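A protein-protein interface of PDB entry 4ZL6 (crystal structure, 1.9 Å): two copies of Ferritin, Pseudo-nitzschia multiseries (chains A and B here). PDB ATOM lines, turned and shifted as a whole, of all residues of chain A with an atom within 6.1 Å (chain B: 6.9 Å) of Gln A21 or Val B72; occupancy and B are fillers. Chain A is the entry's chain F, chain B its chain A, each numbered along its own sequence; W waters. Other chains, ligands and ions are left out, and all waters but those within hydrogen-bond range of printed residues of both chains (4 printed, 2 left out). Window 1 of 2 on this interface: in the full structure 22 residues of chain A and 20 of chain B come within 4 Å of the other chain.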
ATOM      1  N   GLU A  16      -6.487  28.392  15.734  1.00  0.00           N
ATOM      2  CA  GLU A  16      -5.860  29.441  14.907  1.00  0.00           C
ATOM      3  C   GLU A  16      -4.348  29.244  14.864  1.00  0.00           C
ATOM      4  O   GLU A  16      -3.757  29.289  13.791  1.00  0.00           O
ATOM      5  CB  GLU A  16      -6.162  30.807  15.453  1.00  0.00           C
ATOM      6  CG  GLU A  16      -7.645  31.146  15.455  1.00  0.00           C
ATOM      7  CD  GLU A  16      -8.315  31.097  14.083  1.00  0.00           C
ATOM      8  OE1 GLU A  16      -7.642  31.323  13.035  1.00  0.00           O
ATOM      9  OE2 GLU A  16      -9.543  30.874  14.035  1.00  0.00           O
ATOM     10  N   PHE A  17      -3.728  28.994  16.013  1.00  0.00           N
ATOM     11  CA  PHE A  17      -2.258  28.734  16.045  1.00  0.00           C
ATOM     12  C   PHE A  17      -1.850  27.464  15.306  1.00  0.00           C
ATOM     13  O   PHE A  17      -0.809  27.440  14.663  1.00  0.00           O
ATOM     14  CB  PHE A  17      -1.708  28.788  17.469  1.00  0.00           C
ATOM     15  CG  PHE A  17      -1.803  30.132  18.130  1.00  0.00           C
ATOM     16  CD1 PHE A  17      -2.017  31.281  17.412  1.00  0.00           C
ATOM     17  CD2 PHE A  17      -1.635  30.239  19.493  1.00  0.00           C
ATOM     18  CE1 PHE A  17      -2.037  32.524  18.053  1.00  0.00           C
ATOM     19  CE2 PHE A  17      -1.743  31.430  20.148  1.00  0.00           C
ATOM     20  CZ  PHE A  17      -1.943  32.604  19.406  1.00  0.00           C
ATOM     21  N   THR A  18      -2.691  26.422  15.395  1.00  0.00           N
ATOM     22  CA  THR A  18      -2.475  25.174  14.670  1.00  0.00           C
ATOM     23  C   THR A  18      -2.473  25.443  13.192  1.00  0.00           C
ATOM     24  O   THR A  18      -1.539  25.016  12.471  1.00  0.00           O
ATOM     25  CB  THR A  18      -3.538  24.122  15.016  1.00  0.00           C
ATOM     26  OG1 THR A  18      -3.472  23.794  16.390  1.00  0.00           O
ATOM     27  CG2 THR A  18      -3.439  22.909  14.166  1.00  0.00           C
ATOM     28  N   ALA A  19      -3.459  26.224  12.757  1.00  0.00           N
ATOM     29  CA  ALA A  19      -3.615  26.595  11.367  1.00  0.00           C
ATOM     30  C   ALA A  19      -2.388  27.406  10.914  1.00  0.00           C
ATOM     31  O   ALA A  19      -1.839  27.177   9.811  1.00  0.00           O
ATOM     32  CB  ALA A  19      -4.928  27.397  11.101  1.00  0.00           C
ATOM     33  N   SER A  20      -1.944  28.337  11.750  1.00  0.00           N
ATOM     34  CA  SER A  20      -0.736  29.104  11.454  1.00  0.00           C
ATOM     35  C   SER A  20       0.460  28.248  11.137  1.00  0.00           C
ATOM     36  O   SER A  20       1.198  28.517  10.157  1.00  0.00           O
ATOM     37  CB  SER A  20      -0.408  30.093  12.597  1.00  0.00           C
ATOM     38  OG  SER A  20       0.722  30.872  12.264  1.00  0.00           O
ATOM     39  N   GLN A  21       0.642  27.171  11.920  1.00  0.00           N
ATOM     40  CA  GLN A  21       1.730  26.289  11.714  1.00  0.00           C
ATOM     41  C   GLN A  21       1.561  25.435  10.466  1.00  0.00           C
ATOM     42  O   GLN A  21       2.543  25.102   9.783  1.00  0.00           O
ATOM     43  CB  GLN A  21       1.905  25.407  12.952  1.00  0.00           C
ATOM     44  CG  GLN A  21       2.419  26.108  14.134  1.00  0.00           C
ATOM     45  CD  GLN A  21       3.844  26.582  13.950  1.00  0.00           C
ATOM     46  OE1 GLN A  21       4.048  27.719  13.549  1.00  0.00           O
ATOM     47  NE2 GLN A  21       4.843  25.707  14.243  1.00  0.00           N
ATOM     48  N   VAL A  22       0.332  25.039  10.170  1.00  0.00           N
ATOM     49  CA  VAL A  22       0.058  24.292   8.947  1.00  0.00           C
ATOM     50  C   VAL A  22       0.412  25.150   7.697  1.00  0.00           C
ATOM     51  O   VAL A  22       1.074  24.684   6.747  1.00  0.00           O
ATOM     52  CB  VAL A  22      -1.383  23.726   8.887  1.00  0.00           C
ATOM     53  CG1 VAL A  22      -1.696  23.026   7.567  1.00  0.00           C
ATOM     54  CG2 VAL A  22      -1.611  22.691  10.032  1.00  0.00           C
ATOM     55  N   TYR A  23      -0.039  26.397   7.692  1.00  0.00           N
ATOM     56  CA  TYR A  23       0.370  27.302   6.660  1.00  0.00           C
ATOM     57  C   TYR A  23       1.861  27.448   6.541  1.00  0.00           C
ATOM     58  O   TYR A  23       2.356  27.473   5.403  1.00  0.00           O
ATOM     59  CB  TYR A  23      -0.326  28.687   6.800  1.00  0.00           C
ATOM     60  CG  TYR A  23      -1.741  28.733   6.294  1.00  0.00           C
ATOM     61  CD1 TYR A  23      -1.999  28.836   4.911  1.00  0.00           C
ATOM     62  CD2 TYR A  23      -2.831  28.737   7.149  1.00  0.00           C
ATOM     63  CE1 TYR A  23      -3.254  28.907   4.420  1.00  0.00           C
ATOM     64  CE2 TYR A  23      -4.136  28.803   6.664  1.00  0.00           C
ATOM     65  CZ  TYR A  23      -4.343  28.945   5.294  1.00  0.00           C
ATOM     66  OH  TYR A  23      -5.618  29.009   4.820  1.00  0.00           O
ATOM     67  N   LEU A  24       2.587  27.566   7.673  1.00  0.00           N
ATOM     68  CA  LEU A  24       4.038  27.656   7.621  1.00  0.00           C
ATOM     69  C   LEU A  24       4.659  26.376   6.970  1.00  0.00           C
ATOM     70  O   LEU A  24       5.562  26.422   6.129  1.00  0.00           O
ATOM     71  CB  LEU A  24       4.569  27.910   9.034  1.00  0.00           C
ATOM     72  CG  LEU A  24       6.080  27.993   9.089  1.00  0.00           C
ATOM     73  CD1 LEU A  24       6.613  29.169   8.264  1.00  0.00           C
ATOM     74  CD2 LEU A  24       6.497  28.188  10.529  1.00  0.00           C
ATOM     75  N   SER A  25       4.135  25.230   7.349  1.00  0.00           N
ATOM     76  CA  SER A  25       4.557  23.966   6.788  1.00  0.00           C
ATOM     77  C   SER A  25       4.332  23.942   5.263  1.00  0.00           C
ATOM     78  O   SER A  25       5.217  23.507   4.508  1.00  0.00           O
ATOM     79  CB  SER A  25       3.809  22.822   7.461  1.00  0.00           C
ATOM     80  OG  SER A  25       4.255  21.632   6.877  1.00  0.00           O
ATOM     81  N   ALA A  26       3.182  24.424   4.805  1.00  0.00           N
ATOM     82  CA  ALA A  26       2.895  24.532   3.371  1.00  0.00           C
ATOM     83  C   ALA A  26       3.924  25.442   2.699  1.00  0.00           C
ATOM     84  O   ALA A  26       4.404  25.133   1.613  1.00  0.00           O
ATOM     85  CB  ALA A  26       1.484  25.056   3.164  1.00  0.00           C
ATOM     86  N   SER A  46      -0.088  32.313   7.108  1.00  0.00           N
ATOM     87  CA  SER A  46       0.371  31.851   8.419  1.00  0.00           C
ATOM     88  C   SER A  46       0.290  33.004   9.416  1.00  0.00           C
ATOM     89  O   SER A  46      -0.124  32.842  10.577  1.00  0.00           O
ATOM     90  CB  SER A  46       1.783  31.283   8.304  1.00  0.00           C
ATOM     91  OG  SER A  46       2.362  30.941   9.557  1.00  0.00           O
ATOM     92  N   GLN A  70      -2.338  26.120  24.886  1.00  0.00           N
ATOM     93  CA  GLN A  70      -2.128  24.680  24.706  1.00  0.00           C
ATOM     94  C   GLN A  70      -0.958  24.445  23.759  1.00  0.00           C
ATOM     95  O   GLN A  70      -0.504  25.356  23.076  1.00  0.00           O
ATOM     96  CB  GLN A  70      -3.384  23.990  24.166  1.00  0.00           C
ATOM     97  CG  GLN A  70      -4.670  24.297  24.997  1.00  0.00           C
ATOM     98  CD  GLN A  70      -5.929  23.583  24.402  1.00  0.00           C
ATOM     99  OE1 GLN A  70      -6.438  23.838  23.251  1.00  0.00           O
ATOM    100  NE2 GLN A  70      -6.431  22.632  25.189  1.00  0.00           N
ATOM    101  N   ALA A  71      -0.463  23.202  23.758  1.00  0.00           N
ATOM    102  CA  ALA A  71       0.560  22.822  22.798  1.00  0.00           C
ATOM    103  C   ALA A  71       0.012  23.106  21.402  1.00  0.00           C
ATOM    104  O   ALA A  71      -1.152  22.812  21.127  1.00  0.00           O
ATOM    105  CB  ALA A  71       0.856  21.299  22.901  1.00  0.00           C
ATOM    106  N   VAL A  72       0.869  23.589  20.488  1.00  0.00           N
ATOM    107  CA  VAL A  72       0.499  23.763  19.103  1.00  0.00           C
ATOM    108  C   VAL A  72       1.042  22.574  18.344  1.00  0.00           C
ATOM    109  O   VAL A  72       2.223  22.385  18.304  1.00  0.00           O
ATOM    110  CB  VAL A  72       1.068  25.064  18.484  1.00  0.00           C
ATOM    111  CG1 VAL A  72       0.456  25.204  17.065  1.00  0.00           C
ATOM    112  CG2 VAL A  72       0.691  26.237  19.386  1.00  0.00           C
ATOM    113  N   PRO A  73       0.168  21.685  17.906  1.00  0.00           N
ATOM    114  CA  PRO A  73       0.694  20.423  17.391  1.00  0.00           C
ATOM    115  C   PRO A  73       1.603  20.578  16.200  1.00  0.00           C
ATOM    116  O   PRO A  73       1.462  21.533  15.409  1.00  0.00           O
ATOM    117  CB  PRO A  73      -0.558  19.674  16.911  1.00  0.00           C
ATOM    118  CG  PRO A  73      -1.717  20.363  17.528  1.00  0.00           C
ATOM    119  CD  PRO A  73      -1.304  21.768  17.873  1.00  0.00           C
ATOM    120  N   ALA A  74       2.436  19.585  16.015  1.00  0.00           N
ATOM    121  CA  ALA A  74       3.261  19.469  14.854  1.00  0.00           C
ATOM    122  C   ALA A  74       2.381  19.277  13.628  1.00  0.00           C
ATOM    123  O   ALA A  74       1.535  18.396  13.647  1.00  0.00           O
ATOM    124  CB  ALA A  74       4.189  18.292  14.971  1.00  0.00           C
ATOM    125  N   PRO A  75       2.631  20.052  12.546  1.00  0.00           N
ATOM    126  CA  PRO A  75       1.889  19.834  11.287  1.00  0.00           C
ATOM    127  C   PRO A  75       2.352  18.551  10.661  1.00  0.00           C
ATOM    128  O   PRO A  75       3.497  18.257  10.682  1.00  0.00           O
ATOM    129  CB  PRO A  75       2.197  21.077  10.429  1.00  0.00           C
ATOM    130  CG  PRO A  75       3.249  21.831  11.142  1.00  0.00           C
ATOM    131  CD  PRO A  75       3.521  21.226  12.512  1.00  0.00           C
ATOM    132  N   VAL B  13      14.690  26.665  15.611  1.00  0.00           N
ATOM    133  CA  VAL B  13      13.354  27.055  15.178  1.00  0.00           C
ATOM    134  C   VAL B  13      12.285  26.772  16.263  1.00  0.00           C
ATOM    135  O   VAL B  13      11.492  27.631  16.650  1.00  0.00           O
ATOM    136  CB  VAL B  13      12.981  26.349  13.854  1.00  0.00           C
ATOM    137  CG1 VAL B  13      11.503  26.540  13.533  1.00  0.00           C
ATOM    138  CG2 VAL B  13      13.837  26.845  12.707  1.00  0.00           C
ATOM    139  N   THR B  14      12.277  25.534  16.770  1.00  0.00           N
ATOM    140  CA  THR B  14      11.338  25.209  17.837  1.00  0.00           C
ATOM    141  C   THR B  14      11.548  26.095  19.082  1.00  0.00           C
ATOM    142  O   THR B  14      10.577  26.510  19.727  1.00  0.00           O
ATOM    143  CB  THR B  14      11.599  23.743  18.278  1.00  0.00           C
ATOM    144  OG1 THR B  14      11.510  22.913  17.141  1.00  0.00           O
ATOM    145  CG2 THR B  14      10.627  23.340  19.374  1.00  0.00           C
ATOM    146  N   GLU B  16      12.685  29.173  19.160  1.00  0.00           N
ATOM    147  CA  GLU B  16      12.152  30.509  18.894  1.00  0.00           C
ATOM    148  C   GLU B  16      10.637  30.522  18.998  1.00  0.00           C
ATOM    149  O   GLU B  16      10.057  31.440  19.662  1.00  0.00           O
ATOM    150  CB  GLU B  16      12.557  31.033  17.539  1.00  0.00           C
ATOM    151  CG  GLU B  16      14.060  31.175  17.315  1.00  0.00           C
ATOM    152  CD  GLU B  16      14.711  32.213  18.224  1.00  0.00           C
ATOM    153  OE1 GLU B  16      14.016  33.095  18.762  1.00  0.00           O
ATOM    154  OE2 GLU B  16      15.904  32.096  18.441  1.00  0.00           O
ATOM    155  N   PHE B  17       9.974  29.513  18.468  1.00  0.00           N
ATOM    156  CA  PHE B  17       8.502  29.524  18.570  1.00  0.00           C
ATOM    157  C   PHE B  17       8.025  29.228  19.996  1.00  0.00           C
ATOM    158  O   PHE B  17       7.003  29.783  20.481  1.00  0.00           O
ATOM    159  CB  PHE B  17       7.933  28.523  17.612  1.00  0.00           C
ATOM    160  CG  PHE B  17       8.140  28.843  16.153  1.00  0.00           C
ATOM    161  CD1 PHE B  17       8.491  30.137  15.686  1.00  0.00           C
ATOM    162  CD2 PHE B  17       7.980  27.848  15.234  1.00  0.00           C
ATOM    163  CE1 PHE B  17       8.556  30.407  14.334  1.00  0.00           C
ATOM    164  CE2 PHE B  17       8.149  28.088  13.872  1.00  0.00           C
ATOM    165  CZ  PHE B  17       8.479  29.381  13.416  1.00  0.00           C
ATOM    166  N   THR B  18       8.779  28.381  20.699  1.00  0.00           N
ATOM    167  CA  THR B  18       8.556  28.143  22.122  1.00  0.00           C
ATOM    168  C   THR B  18       8.601  29.421  22.948  1.00  0.00           C
ATOM    169  O   THR B  18       7.687  29.729  23.721  1.00  0.00           O
ATOM    170  CB  THR B  18       9.536  27.116  22.698  1.00  0.00           C
ATOM    171  OG1 THR B  18       9.318  25.877  22.055  1.00  0.00           O
ATOM    172  CG2 THR B  18       9.382  26.910  24.172  1.00  0.00           C
ATOM    173  N   ALA B  19       9.624  30.192  22.727  1.00  0.00           N
ATOM    174  CA  ALA B  19       9.791  31.481  23.375  1.00  0.00           C
ATOM    175  C   ALA B  19       8.686  32.468  23.008  1.00  0.00           C
ATOM    176  O   ALA B  19       8.167  33.214  23.894  1.00  0.00           O
ATOM    177  CB  ALA B  19      11.211  32.061  23.075  1.00  0.00           C
ATOM    178  N   SER B  20       8.255  32.445  21.746  1.00  0.00           N
ATOM    179  CA  SER B  20       7.111  33.267  21.318  1.00  0.00           C
ATOM    180  C   SER B  20       5.880  32.984  22.149  1.00  0.00           C
ATOM    181  O   SER B  20       5.193  33.881  22.577  1.00  0.00           O
ATOM    182  CB  SER B  20       6.800  33.078  19.847  1.00  0.00           C
ATOM    183  OG  SER B  20       5.777  33.910  19.479  1.00  0.00           O
ATOM    184  N   GLN B  21       5.597  31.712  22.404  1.00  0.00           N
ATOM    185  CA  GLN B  21       4.479  31.357  23.221  1.00  0.00           C
ATOM    186  C   GLN B  21       4.650  31.774  24.647  1.00  0.00           C
ATOM    187  O   GLN B  21       3.702  32.185  25.299  1.00  0.00           O
ATOM    188  CB  GLN B  21       4.198  29.834  23.166  1.00  0.00           C
ATOM    189  CG  GLN B  21       3.667  29.405  21.851  1.00  0.00           C
ATOM    190  CD  GLN B  21       2.232  29.875  21.609  1.00  0.00           C
ATOM    191  OE1 GLN B  21       2.016  30.951  21.089  1.00  0.00           O
ATOM    192  NE2 GLN B  21       1.269  29.047  21.930  1.00  0.00           N
ATOM    193  N   ARG B  50       8.792  35.058  17.053  1.00  0.00           N
ATOM    194  CA  ARG B  50       8.302  34.321  15.895  1.00  0.00           C
ATOM    195  C   ARG B  50       9.052  34.745  14.621  1.00  0.00           C
ATOM    196  O   ARG B  50       9.461  33.887  13.803  1.00  0.00           O
ATOM    197  CB  ARG B  50       6.810  34.541  15.732  1.00  0.00           C
ATOM    198  CG  ARG B  50       6.259  33.769  14.555  1.00  0.00           C
ATOM    199  CD  ARG B  50       4.775  33.593  14.593  1.00  0.00           C
ATOM    200  NE  ARG B  50       4.273  33.049  13.324  1.00  0.00           N
ATOM    201  CZ  ARG B  50       4.061  33.792  12.220  1.00  0.00           C
ATOM    202  NH1 ARG B  50       4.337  35.091  12.173  1.00  0.00           N
ATOM    203  NH2 ARG B  50       3.657  33.216  11.143  1.00  0.00           N
ATOM    204  N   LEU B  54      11.099  32.456  11.953  1.00  0.00           N
ATOM    205  CA  LEU B  54      10.859  32.525  10.509  1.00  0.00           C
ATOM    206  C   LEU B  54      12.148  32.776   9.726  1.00  0.00           C
ATOM    207  O   LEU B  54      12.345  32.243   8.598  1.00  0.00           O
ATOM    208  CB  LEU B  54       9.810  33.586  10.190  1.00  0.00           C
ATOM    209  CG  LEU B  54       8.429  33.222  10.743  1.00  0.00           C
ATOM    210  CD1 LEU B  54       7.510  34.398  10.455  1.00  0.00           C
ATOM    211  CD2 LEU B  54       7.781  32.027  10.079  1.00  0.00           C
ATOM    212  N   LEU B  69       8.875  20.943  11.221  1.00  0.00           N
ATOM    213  CA  LEU B  69       8.247  21.696  12.291  1.00  0.00           C
ATOM    214  C   LEU B  69       7.799  20.780  13.396  1.00  0.00           C
ATOM    215  O   LEU B  69       7.016  19.811  13.138  1.00  0.00           O
ATOM    216  CB  LEU B  69       7.053  22.469  11.763  1.00  0.00           C
ATOM    217  CG  LEU B  69       7.455  23.591  10.762  1.00  0.00           C
ATOM    218  CD1 LEU B  69       6.252  24.271  10.263  1.00  0.00           C
ATOM    219  CD2 LEU B  69       8.430  24.557  11.461  1.00  0.00           C
ATOM    220  N   GLN B  70       8.262  21.034  14.595  1.00  0.00           N
ATOM    221  CA  GLN B  70       7.807  20.245  15.757  1.00  0.00           C
ATOM    222  C   GLN B  70       6.646  20.923  16.468  1.00  0.00           C
ATOM    223  O   GLN B  70       6.288  22.113  16.161  1.00  0.00           O
ATOM    224  CB  GLN B  70       8.976  20.123  16.714  1.00  0.00           C
ATOM    225  CG  GLN B  70      10.291  19.636  16.037  1.00  0.00           C
ATOM    226  CD  GLN B  70      10.218  18.193  15.626  1.00  0.00           C
ATOM    227  OE1 GLN B  70      10.034  17.337  16.467  1.00  0.00           O
ATOM    228  NE2 GLN B  70      10.346  17.907  14.334  1.00  0.00           N
ATOM    229  N   ALA B  71       6.041  20.193  17.411  1.00  0.00           N
ATOM    230  CA  ALA B  71       5.121  20.814  18.319  1.00  0.00           C
ATOM    231  C   ALA B  71       5.753  22.006  19.046  1.00  0.00           C
ATOM    232  O   ALA B  71       6.941  22.008  19.344  1.00  0.00           O
ATOM    233  CB  ALA B  71       4.612  19.801  19.351  1.00  0.00           C
ATOM    234  N   VAL B  72       4.928  23.021  19.299  1.00  0.00           N
ATOM    235  CA  VAL B  72       5.317  24.104  20.120  1.00  0.00           C
ATOM    236  C   VAL B  72       4.698  23.886  21.506  1.00  0.00           C
ATOM    237  O   VAL B  72       3.461  23.996  21.655  1.00  0.00           O
ATOM    238  CB  VAL B  72       4.885  25.460  19.555  1.00  0.00           C
ATOM    239  CG1 VAL B  72       5.520  26.578  20.386  1.00  0.00           C
ATOM    240  CG2 VAL B  72       5.244  25.614  18.069  1.00  0.00           C
ATOM    241  N   PRO B  73       5.544  23.545  22.511  1.00  0.00           N
ATOM    242  CA  PRO B  73       5.014  23.118  23.809  1.00  0.00           C
ATOM    243  C   PRO B  73       4.289  24.219  24.506  1.00  0.00           C
ATOM    244  O   PRO B  73       4.566  25.395  24.266  1.00  0.00           O
ATOM    245  CB  PRO B  73       6.233  22.688  24.609  1.00  0.00           C
ATOM    246  CG  PRO B  73       7.275  22.378  23.551  1.00  0.00           C
ATOM    247  CD  PRO B  73       7.023  23.406  22.457  1.00  0.00           C
ATOM    248  N   ALA B  74       3.261  23.833  25.233  1.00  0.00           N
ATOM    249  CA  ALA B  74       2.470  24.759  26.004  1.00  0.00           C
ATOM    250  C   ALA B  74       3.431  25.389  27.040  1.00  0.00           C
ATOM    251  O   ALA B  74       4.221  24.677  27.728  1.00  0.00           O
ATOM    252  CB  ALA B  74       1.348  24.008  26.748  1.00  0.00           C
ATOM    253  N   PRO B  75       3.332  26.687  27.231  1.00  0.00           N
ATOM    254  CA  PRO B  75       4.082  27.407  28.306  1.00  0.00           C
ATOM    255  C   PRO B  75       3.559  26.976  29.665  1.00  0.00           C
ATOM    256  O   PRO B  75       2.391  26.751  29.782  1.00  0.00           O
ATOM    257  CB  PRO B  75       3.716  28.882  28.103  1.00  0.00           C
ATOM    258  CG  PRO B  75       3.018  28.954  26.862  1.00  0.00           C
ATOM    259  CD  PRO B  75       2.558  27.585  26.383  1.00  0.00           C
HETATM  260  O   HOH W   1       3.413  30.269  12.633  1.00  0.00           O
HETATM  261  O   HOH W   2      -1.345  27.841  22.021  1.00  0.00           O
HETATM  262  O   HOH W   3       6.080  18.692  10.949  1.00  0.00           O
HETATM  263  O   HOH W   4       7.495  24.489  15.148  1.00  0.00           O
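The guanidinium group (NH2) of Arg B50 is in hydrogen-bond range of the side-chain hydroxyl (OG) of Ser A46, 3.1 Å away.
O of Val B72 sits at hydrogen-bond distance from N of Val A72 (2.9 Å).
The backbone carbonyl oxygen (O) of Ser A46 is in hydrogen-bond range of the side-chain hydroxyl (OG) of Ser A20.
Phe A17 touches Gln B21.
Arg B50 touches Ser A20 (NH2 to OG, 3.9 Å).
Val B72 touches Gln A21 (CG2 to NE2, 3.8 Å).
CZ of Phe B17 touches CD2 of Leu A24 (3.7 Å).
Leu A24 touches Leu B54 (CD1 to CD2, 3.6 Å).
Leu B69 touches Leu A24 (CD1 to CG, 3.9 Å).
Val B72 touches Ala A71 (O to CA, 3.3 Å).
Val A72 touches Gln B21.
CB of Ala A74 touches N of Ala B71, at 3.6 Å.
CD of Pro A75 touches CB of Leu B69 (3.8 Å).
Of the printed residues of chain B, Ser A20 touches Arg B50.
Gln A21 touches just these residues of chain B: Phe B17 (3.9 Å), Leu B69 (3.8 Å) and Val B72 (3.8 Å).
Of the printed residues of chain B, Leu A24 touches Phe B17, Leu B54 and Leu B69.
Of chain A, only Gln A21, Ala A71 and Val A72 come within 4 Å of Val B72.
The nearest printed residue of chain A that does not touch Leu B54 is Ser A46 (5.6 Å).
Of the 18 printed residues of chain A, 11 touch a printed residue of chain B.
Among the printed residues, 20 pairs touch across the chains.
Among the printed residues, no Asp or Glu carboxylate lies within 4 Å of a Lys or Arg side-chain nitrogen of the other chain.
Gln A21 touches Val B72, and with the chains exchanged Val A72 touches Gln B21.
Gln A70 touches Ala B74, and with the chains exchanged Ala A74 touches Gln B70.
Ala A71 touches Ala B74, and with the chains exchanged Ala A74 touches Ala B71.
Val B72 touches its own counterpart, Val A72.
Water W3 bridges O of Leu B69 (2.6 Å) and O of Pro A75 (2.6 Å).
Water W1 lies within hydrogen-bond range of OE1 of Gln A21 (2.8 Å), OG of Ser A20 (2.8 Å), NE of Arg B50 (3.0 Å) and OG of Ser A46 (3.3 Å).
Water W2 bridges O of Gln A70 and NE2 of Gln B21.
Water W4 bridges the backbone carbonyl oxygen of Gln B70 (2.9 Å) and the side-chain amide nitrogen of Gln A21 (3.1 Å).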
